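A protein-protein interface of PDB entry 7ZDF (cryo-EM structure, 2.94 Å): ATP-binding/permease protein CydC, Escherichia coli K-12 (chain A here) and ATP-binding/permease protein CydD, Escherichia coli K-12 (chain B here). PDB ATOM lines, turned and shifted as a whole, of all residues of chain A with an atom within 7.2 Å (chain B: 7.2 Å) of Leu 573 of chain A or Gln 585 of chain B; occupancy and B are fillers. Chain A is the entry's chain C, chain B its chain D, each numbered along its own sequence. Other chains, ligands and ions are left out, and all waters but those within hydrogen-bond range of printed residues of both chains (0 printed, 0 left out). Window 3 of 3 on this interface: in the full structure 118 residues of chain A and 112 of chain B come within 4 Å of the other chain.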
ATOM      1  N   ARG A 374      -3.696 -29.557  27.280  1.00  0.00           N
ATOM      2  CA  ARG A 374      -2.413 -29.834  26.653  1.00  0.00           C
ATOM      3  C   ARG A 374      -2.615 -30.103  25.168  1.00  0.00           C
ATOM      4  O   ARG A 374      -3.592 -30.738  24.763  1.00  0.00           O
ATOM      5  CB  ARG A 374      -1.716 -31.026  27.314  1.00  0.00           C
ATOM      6  CG  ARG A 374      -0.204 -31.003  27.180  1.00  0.00           C
ATOM      7  CD  ARG A 374       0.424 -32.258  27.756  1.00  0.00           C
ATOM      8  NE  ARG A 374       0.400 -32.258  29.215  1.00  0.00           N
ATOM      9  CZ  ARG A 374       1.275 -31.611  29.978  1.00  0.00           C
ATOM     10  NH1 ARG A 374       2.252 -30.909  29.423  1.00  0.00           N
ATOM     11  NH2 ARG A 374       1.173 -31.669  31.298  1.00  0.00           N
ATOM     12  N   ARG A 532      -2.506 -22.242  26.076  1.00  0.00           N
ATOM     13  CA  ARG A 532      -1.532 -21.159  25.968  1.00  0.00           C
ATOM     14  C   ARG A 532      -1.603 -20.299  27.220  1.00  0.00           C
ATOM     15  O   ARG A 532      -2.640 -19.690  27.496  1.00  0.00           O
ATOM     16  CB  ARG A 532      -1.795 -20.306  24.725  1.00  0.00           C
ATOM     17  CG  ARG A 532      -1.134 -20.798  23.457  1.00  0.00           C
ATOM     18  CD  ARG A 532      -0.988 -19.645  22.474  1.00  0.00           C
ATOM     19  NE  ARG A 532      -0.354 -18.469  23.070  1.00  0.00           N
ATOM     20  CZ  ARG A 532       0.956 -18.271  23.159  1.00  0.00           C
ATOM     21  NH1 ARG A 532       1.804 -19.162  22.683  1.00  0.00           N
ATOM     22  NH2 ARG A 532       1.422 -17.165  23.717  1.00  0.00           N
ATOM     23  N   LEU A 533      -0.498 -20.236  27.964  1.00  0.00           N
ATOM     24  CA  LEU A 533      -0.457 -19.511  29.228  1.00  0.00           C
ATOM     25  C   LEU A 533      -0.180 -18.028  29.033  1.00  0.00           C
ATOM     26  O   LEU A 533       0.753 -17.487  29.635  1.00  0.00           O
ATOM     27  CB  LEU A 533       0.607 -20.103  30.153  1.00  0.00           C
ATOM     28  CG  LEU A 533       0.308 -21.400  30.899  1.00  0.00           C
ATOM     29  CD1 LEU A 533       0.302 -22.583  29.959  1.00  0.00           C
ATOM     30  CD2 LEU A 533       1.340 -21.595  31.981  1.00  0.00           C
ATOM     31  N   ARG A 565       0.553 -28.114  39.302  1.00  0.00           N
ATOM     32  CA  ARG A 565       0.750 -28.374  37.879  1.00  0.00           C
ATOM     33  C   ARG A 565       0.912 -27.077  37.095  1.00  0.00           C
ATOM     34  O   ARG A 565       1.755 -26.987  36.195  1.00  0.00           O
ATOM     35  CB  ARG A 565      -0.429 -29.183  37.340  1.00  0.00           C
ATOM     36  CG  ARG A 565      -0.399 -29.505  35.851  1.00  0.00           C
ATOM     37  CD  ARG A 565       0.667 -30.527  35.473  1.00  0.00           C
ATOM     38  NE  ARG A 565       1.980 -29.938  35.234  1.00  0.00           N
ATOM     39  CZ  ARG A 565       3.087 -30.649  35.048  1.00  0.00           C
ATOM     40  NH1 ARG A 565       3.037 -31.973  35.073  1.00  0.00           N
ATOM     41  NH2 ARG A 565       4.243 -30.041  34.830  1.00  0.00           N
ATOM     42  N   GLN A 568       4.465 -25.526  37.486  1.00  0.00           N
ATOM     43  CA  GLN A 568       5.468 -26.140  36.623  1.00  0.00           C
ATOM     44  C   GLN A 568       5.339 -25.638  35.192  1.00  0.00           C
ATOM     45  O   GLN A 568       6.343 -25.485  34.486  1.00  0.00           O
ATOM     46  CB  GLN A 568       5.341 -27.663  36.663  1.00  0.00           C
ATOM     47  CG  GLN A 568       5.147 -28.261  38.048  1.00  0.00           C
ATOM     48  CD  GLN A 568       6.186 -27.791  39.046  1.00  0.00           C
ATOM     49  OE1 GLN A 568       5.955 -26.849  39.801  1.00  0.00           O
ATOM     50  NE2 GLN A 568       7.339 -28.449  39.053  1.00  0.00           N
ATOM     51  N   PHE A 569       4.111 -25.323  34.770  1.00  0.00           N
ATOM     52  CA  PHE A 569       3.915 -24.778  33.401  1.00  0.00           C
ATOM     53  C   PHE A 569       4.757 -23.506  33.259  1.00  0.00           C
ATOM     54  O   PHE A 569       5.606 -23.449  32.353  1.00  0.00           O
ATOM     55  CB  PHE A 569       2.431 -24.550  33.105  1.00  0.00           C
ATOM     56  CG  PHE A 569       1.662 -25.809  32.803  1.00  0.00           C
ATOM     57  CD1 PHE A 569       0.298 -25.883  33.025  1.00  0.00           C
ATOM     58  CD2 PHE A 569       2.308 -26.931  32.310  1.00  0.00           C
ATOM     59  CE1 PHE A 569      -0.405 -27.043  32.747  1.00  0.00           C
ATOM     60  CE2 PHE A 569       1.605 -28.092  32.035  1.00  0.00           C
ATOM     61  CZ  PHE A 569       0.250 -28.146  32.254  1.00  0.00           C
ATOM     62  N   LYS A 570       4.527 -22.523  34.131  1.00  0.00           N
ATOM     63  CA  LYS A 570       5.326 -21.270  34.113  1.00  0.00           C
ATOM     64  C   LYS A 570       6.783 -21.531  34.534  1.00  0.00           C
ATOM     65  O   LYS A 570       7.690 -21.051  33.829  1.00  0.00           O
ATOM     66  CB  LYS A 570       4.697 -20.264  35.081  1.00  0.00           C
ATOM     67  CG  LYS A 570       3.188 -20.096  34.963  1.00  0.00           C
ATOM     68  CD  LYS A 570       2.783 -19.003  34.001  1.00  0.00           C
ATOM     69  CE  LYS A 570       3.254 -17.634  34.443  1.00  0.00           C
ATOM     70  NZ  LYS A 570       2.803 -16.573  33.516  1.00  0.00           N
ATOM     71  N   GLN A 571       6.994 -22.278  35.627  1.00  0.00           N
ATOM     72  CA  GLN A 571       8.359 -22.527  36.180  1.00  0.00           C
ATOM     73  C   GLN A 571       9.238 -23.403  35.276  1.00  0.00           C
ATOM     74  O   GLN A 571      10.386 -23.000  35.014  1.00  0.00           O
ATOM     75  CB  GLN A 571       8.258 -23.135  37.579  1.00  0.00           C
ATOM     76  CG  GLN A 571       7.918 -22.113  38.652  1.00  0.00           C
ATOM     77  CD  GLN A 571       8.796 -20.890  38.551  1.00  0.00           C
ATOM     78  OE1 GLN A 571       9.750 -20.850  37.780  1.00  0.00           O
ATOM     79  NE2 GLN A 571       8.475 -19.876  39.337  1.00  0.00           N
ATOM     80  N   GLY A 572       8.703 -24.521  34.779  1.00  0.00           N
ATOM     81  CA  GLY A 572       9.459 -25.449  33.912  1.00  0.00           C
ATOM     82  C   GLY A 572       9.076 -25.228  32.463  1.00  0.00           C
ATOM     83  O   GLY A 572       8.665 -24.077  32.181  1.00  0.00           O
ATOM     84  N   LEU A 573       8.990 -26.323  31.682  1.00  0.00           N
ATOM     85  CA  LEU A 573       8.872 -26.316  30.197  1.00  0.00           C
ATOM     86  C   LEU A 573       9.401 -24.988  29.647  1.00  0.00           C
ATOM     87  O   LEU A 573      10.360 -25.046  28.851  1.00  0.00           O
ATOM     88  CB  LEU A 573       7.409 -26.537  29.796  1.00  0.00           C
ATOM     89  CG  LEU A 573       6.819 -27.902  30.145  1.00  0.00           C
ATOM     90  CD1 LEU A 573       7.043 -28.236  31.612  1.00  0.00           C
ATOM     91  CD2 LEU A 573       5.336 -27.951  29.809  1.00  0.00           C
ATOM     92  N   HIS B 542       9.885 -23.848  15.023  1.00  0.00           N
ATOM     93  CA  HIS B 542       9.479 -22.970  16.107  1.00  0.00           C
ATOM     94  C   HIS B 542       9.747 -23.587  17.471  1.00  0.00           C
ATOM     95  O   HIS B 542       9.445 -22.958  18.489  1.00  0.00           O
ATOM     96  CB  HIS B 542       7.992 -22.605  15.989  1.00  0.00           C
ATOM     97  CG  HIS B 542       7.606 -21.389  16.773  1.00  0.00           C
ATOM     98  ND1 HIS B 542       8.124 -20.139  16.512  1.00  0.00           N
ATOM     99  CD2 HIS B 542       6.756 -21.233  17.815  1.00  0.00           C
ATOM    100  CE1 HIS B 542       7.610 -19.264  17.357  1.00  0.00           C
ATOM    101  NE2 HIS B 542       6.776 -19.903  18.160  1.00  0.00           N
ATOM    102  N   LEU B 544      11.919 -23.615  19.781  1.00  0.00           N
ATOM    103  CA  LEU B 544      13.101 -22.820  20.079  1.00  0.00           C
ATOM    104  C   LEU B 544      13.863 -23.315  21.300  1.00  0.00           C
ATOM    105  O   LEU B 544      14.981 -22.847  21.538  1.00  0.00           O
ATOM    106  CB  LEU B 544      12.699 -21.360  20.280  1.00  0.00           C
ATOM    107  CG  LEU B 544      11.851 -20.771  19.153  1.00  0.00           C
ATOM    108  CD1 LEU B 544      11.565 -19.305  19.395  1.00  0.00           C
ATOM    109  CD2 LEU B 544      12.521 -20.972  17.820  1.00  0.00           C
ATOM    110  N   GLU B 545      13.294 -24.237  22.075  1.00  0.00           N
ATOM    111  CA  GLU B 545      13.969 -24.714  23.276  1.00  0.00           C
ATOM    112  C   GLU B 545      15.095 -25.690  22.961  1.00  0.00           C
ATOM    113  O   GLU B 545      16.073 -25.763  23.713  1.00  0.00           O
ATOM    114  CB  GLU B 545      12.957 -25.369  24.219  1.00  0.00           C
ATOM    115  CG  GLU B 545      12.162 -26.502  23.590  1.00  0.00           C
ATOM    116  CD  GLU B 545      10.826 -26.045  23.040  1.00  0.00           C
ATOM    117  OE1 GLU B 545      10.517 -24.840  23.151  1.00  0.00           O
ATOM    118  OE2 GLU B 545      10.085 -26.889  22.494  1.00  0.00           O
ATOM    119  N   TYR B 567      22.298 -20.039  20.485  1.00  0.00           N
ATOM    120  CA  TYR B 567      21.268 -19.991  21.518  1.00  0.00           C
ATOM    121  C   TYR B 567      21.793 -19.369  22.803  1.00  0.00           C
ATOM    122  O   TYR B 567      21.046 -18.700  23.528  1.00  0.00           O
ATOM    123  CB  TYR B 567      20.741 -21.397  21.784  1.00  0.00           C
ATOM    124  CG  TYR B 567      19.589 -21.468  22.756  1.00  0.00           C
ATOM    125  CD1 TYR B 567      18.290 -21.210  22.343  1.00  0.00           C
ATOM    126  CD2 TYR B 567      19.797 -21.806  24.086  1.00  0.00           C
ATOM    127  CE1 TYR B 567      17.235 -21.280  23.227  1.00  0.00           C
ATOM    128  CE2 TYR B 567      18.749 -21.877  24.976  1.00  0.00           C
ATOM    129  CZ  TYR B 567      17.469 -21.613  24.542  1.00  0.00           C
ATOM    130  OH  TYR B 567      16.421 -21.684  25.429  1.00  0.00           O
ATOM    131  N   ALA B 578      14.709 -13.447  21.625  1.00  0.00           N
ATOM    132  CA  ALA B 578      14.189 -13.555  22.985  1.00  0.00           C
ATOM    133  C   ALA B 578      12.680 -13.360  23.010  1.00  0.00           C
ATOM    134  O   ALA B 578      11.971 -14.038  23.761  1.00  0.00           O
ATOM    135  CB  ALA B 578      14.879 -12.541  23.895  1.00  0.00           C
ATOM    136  N   THR B 579      12.172 -12.429  22.198  1.00  0.00           N
ATOM    137  CA  THR B 579      10.728 -12.267  22.075  1.00  0.00           C
ATOM    138  C   THR B 579      10.084 -13.518  21.494  1.00  0.00           C
ATOM    139  O   THR B 579       9.027 -13.957  21.961  1.00  0.00           O
ATOM    140  CB  THR B 579      10.410 -11.047  21.209  1.00  0.00           C
ATOM    141  OG1 THR B 579      10.913  -9.866  21.845  1.00  0.00           O
ATOM    142  CG2 THR B 579       8.910 -10.906  21.013  1.00  0.00           C
ATOM    143  N   LEU B 580      10.708 -14.107  20.471  1.00  0.00           N
ATOM    144  CA  LEU B 580      10.195 -15.351  19.906  1.00  0.00           C
ATOM    145  C   LEU B 580      10.266 -16.486  20.917  1.00  0.00           C
ATOM    146  O   LEU B 580       9.335 -17.293  21.022  1.00  0.00           O
ATOM    147  CB  LEU B 580      10.977 -15.713  18.644  1.00  0.00           C
ATOM    148  CG  LEU B 580      10.664 -14.908  17.386  1.00  0.00           C
ATOM    149  CD1 LEU B 580      11.634 -15.271  16.281  1.00  0.00           C
ATOM    150  CD2 LEU B 580       9.234 -15.151  16.947  1.00  0.00           C
ATOM    151  N   LEU B 581      11.369 -16.574  21.662  1.00  0.00           N
ATOM    152  CA  LEU B 581      11.498 -17.618  22.672  1.00  0.00           C
ATOM    153  C   LEU B 581      10.469 -17.444  23.780  1.00  0.00           C
ATOM    154  O   LEU B 581       9.864 -18.421  24.233  1.00  0.00           O
ATOM    155  CB  LEU B 581      12.912 -17.621  23.248  1.00  0.00           C
ATOM    156  CG  LEU B 581      13.227 -18.728  24.254  1.00  0.00           C
ATOM    157  CD1 LEU B 581      12.851 -20.086  23.695  1.00  0.00           C
ATOM    158  CD2 LEU B 581      14.694 -18.695  24.642  1.00  0.00           C
ATOM    159  N   ALA B 582      10.256 -16.204  24.228  1.00  0.00           N
ATOM    160  CA  ALA B 582       9.285 -15.955  25.289  1.00  0.00           C
ATOM    161  C   ALA B 582       7.881 -16.351  24.856  1.00  0.00           C
ATOM    162  O   ALA B 582       7.128 -16.948  25.635  1.00  0.00           O
ATOM    163  CB  ALA B 582       9.327 -14.485  25.701  1.00  0.00           C
ATOM    164  N   HIS B 583       7.507 -16.023  23.618  1.00  0.00           N
ATOM    165  CA  HIS B 583       6.196 -16.413  23.112  1.00  0.00           C
ATOM    166  C   HIS B 583       6.086 -17.924  22.951  1.00  0.00           C
ATOM    167  O   HIS B 583       4.990 -18.480  23.068  1.00  0.00           O
ATOM    168  CB  HIS B 583       5.924 -15.699  21.787  1.00  0.00           C
ATOM    169  CG  HIS B 583       4.894 -16.369  20.934  1.00  0.00           C
ATOM    170  ND1 HIS B 583       5.216 -17.282  19.952  1.00  0.00           N
ATOM    171  CD2 HIS B 583       3.545 -16.252  20.907  1.00  0.00           C
ATOM    172  CE1 HIS B 583       4.112 -17.702  19.363  1.00  0.00           C
ATOM    173  NE2 HIS B 583       3.083 -17.092  19.923  1.00  0.00           N
ATOM    174  N   ARG B 584       7.206 -18.602  22.691  1.00  0.00           N
ATOM    175  CA  ARG B 584       7.180 -20.054  22.547  1.00  0.00           C
ATOM    176  C   ARG B 584       7.036 -20.756  23.893  1.00  0.00           C
ATOM    177  O   ARG B 584       6.479 -21.858  23.960  1.00  0.00           O
ATOM    178  CB  ARG B 584       8.445 -20.519  21.822  1.00  0.00           C
ATOM    179  CG  ARG B 584       8.775 -21.995  21.977  1.00  0.00           C
ATOM    180  CD  ARG B 584       7.821 -22.861  21.181  1.00  0.00           C
ATOM    181  NE  ARG B 584       8.016 -24.278  21.467  1.00  0.00           N
ATOM    182  CZ  ARG B 584       7.227 -25.245  21.012  1.00  0.00           C
ATOM    183  NH1 ARG B 584       6.186 -24.950  20.248  1.00  0.00           N
ATOM    184  NH2 ARG B 584       7.481 -26.509  21.321  1.00  0.00           N
ATOM    185  N   GLN B 585       7.494 -20.127  24.975  1.00  0.00           N
ATOM    186  CA  GLN B 585       7.471 -20.767  26.284  1.00  0.00           C
ATOM    187  C   GLN B 585       6.064 -20.919  26.846  1.00  0.00           C
ATOM    188  O   GLN B 585       5.895 -21.590  27.869  1.00  0.00           O
ATOM    189  CB  GLN B 585       8.333 -19.977  27.268  1.00  0.00           C
ATOM    190  CG  GLN B 585       9.817 -19.988  26.950  1.00  0.00           C
ATOM    191  CD  GLN B 585      10.516 -21.232  27.453  1.00  0.00           C
ATOM    192  OE1 GLN B 585      10.190 -22.348  27.049  1.00  0.00           O
ATOM    193  NE2 GLN B 585      11.487 -21.046  28.336  1.00  0.00           N
ATOM    194  N   GLU B 586       5.061 -20.318  26.211  1.00  0.00           N
ATOM    195  CA  GLU B 586       3.689 -20.396  26.690  1.00  0.00           C
ATOM    196  C   GLU B 586       2.923 -21.590  26.134  1.00  0.00           C
ATOM    197  O   GLU B 586       1.868 -21.930  26.676  1.00  0.00           O
ATOM    198  CB  GLU B 586       2.968 -19.087  26.369  1.00  0.00           C
ATOM    199  CG  GLU B 586       3.540 -17.919  27.163  1.00  0.00           C
ATOM    200  CD  GLU B 586       3.420 -16.590  26.452  1.00  0.00           C
ATOM    201  OE1 GLU B 586       2.736 -16.530  25.413  1.00  0.00           O
ATOM    202  OE2 GLU B 586       4.019 -15.603  26.932  1.00  0.00           O
ATOM    203  N   GLU B 587       3.453 -22.256  25.109  1.00  0.00           N
ATOM    204  CA  GLU B 587       2.741 -23.439  24.556  1.00  0.00           C
ATOM    205  C   GLU B 587       2.988 -24.655  25.460  1.00  0.00           C
ATOM    206  O   GLU B 587       4.161 -24.935  25.763  1.00  0.00           O
ATOM    207  CB  GLU B 587       3.187 -23.725  23.122  1.00  0.00           C
ATOM    208  CG  GLU B 587       2.553 -24.977  22.542  1.00  0.00           C
ATOM    209  CD  GLU B 587       2.914 -25.267  21.097  1.00  0.00           C
ATOM    210  OE1 GLU B 587       2.917 -26.456  20.719  1.00  0.00           O
ATOM    211  OE2 GLU B 587       3.188 -24.306  20.353  1.00  0.00           O
ATOM    212  N   ILE B 588       1.914 -25.351  25.849  1.00  0.00           N
ATOM    213  CA  ILE B 588       1.980 -26.538  26.688  1.00  0.00           C
ATOM    214  C   ILE B 588       1.227 -27.669  25.997  1.00  0.00           C
ATOM    215  O   ILE B 588       0.284 -27.429  25.239  1.00  0.00           O
ATOM    216  CB  ILE B 588       1.411 -26.288  28.095  1.00  0.00           C
ATOM    217  CG1 ILE B 588       0.001 -25.712  28.012  1.00  0.00           C
ATOM    218  CG2 ILE B 588       2.320 -25.367  28.891  1.00  0.00           C
ATOM    219  CD1 ILE B 588      -0.809 -25.973  29.249  1.00  0.00           C
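The side-chain amide oxygen (OE1) of Gln 585 of chain B sits close to the backbone carbonyl oxygen (O) of Leu 573 of chain A (3.2 Å). The guanidinium group of Arg 532 of chain A is in salt-bridge range of the side-chain carboxylate of Glu 586 of chain B, at 3.9 Å. The backbone carbonyl oxygen (O) of His 583 of chain B lies within hydrogen-bond range of the guanidinium group (NH1) of Arg 532 of chain A. The backbone NH (N) of Leu 533 of chain A is in hydrogen-bond range of the backbone carbonyl oxygen (O) of Glu 586 of chain B.
Arg 374 of chain A touches Ile 588 of chain B. Ile 588 of chain B touches Leu 533 of chain A (CG2 to CD1, 3.6 Å). Phe 569 of chain A touches Ile 588 of chain B.
Printed residues of chain B within 4 Å of Arg 374 of chain A: Ile 588 (3.8 Å). Arg 565 of chain A touches none of the printed residues of chain B. Printed residues of chain B within 4 Å of Leu 573 of chain A: Gln 585. Ala 578 of chain B touches none of the printed residues of chain A. Printed residues of chain A within 4 Å of His 583 of chain B: Arg 532 (3.3 Å). Gln 585 of chain B touches just one residue of chain A: Leu 573 (3.2 Å). The nearest residue of chain B that does not touch Leu 573 of chain A is Ile 588 of chain B (4.1 Å). The nearest printed residue of chain B that does not touch Arg 532 of chain A is Glu 587 of chain B (4.3 Å).
Of the 10 printed residues of chain A, 5 touch a printed residue of chain B. Along chain A the printed residues that touch a printed residue of chain B span positions 374 to 573. Printed residues of chain B that touch a printed residue of chain A: His 583, Gln 585, Glu 586 and Ile 588. Hydrophobic or aromatic side chains of chain B within 4 Å of the printed part of chain A: His 583 and Ile 588. Along chain B the printed residues that touch a printed residue of chain A span positions 583 to 588. Among the printed residues, 7 pairs touch across the chains.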
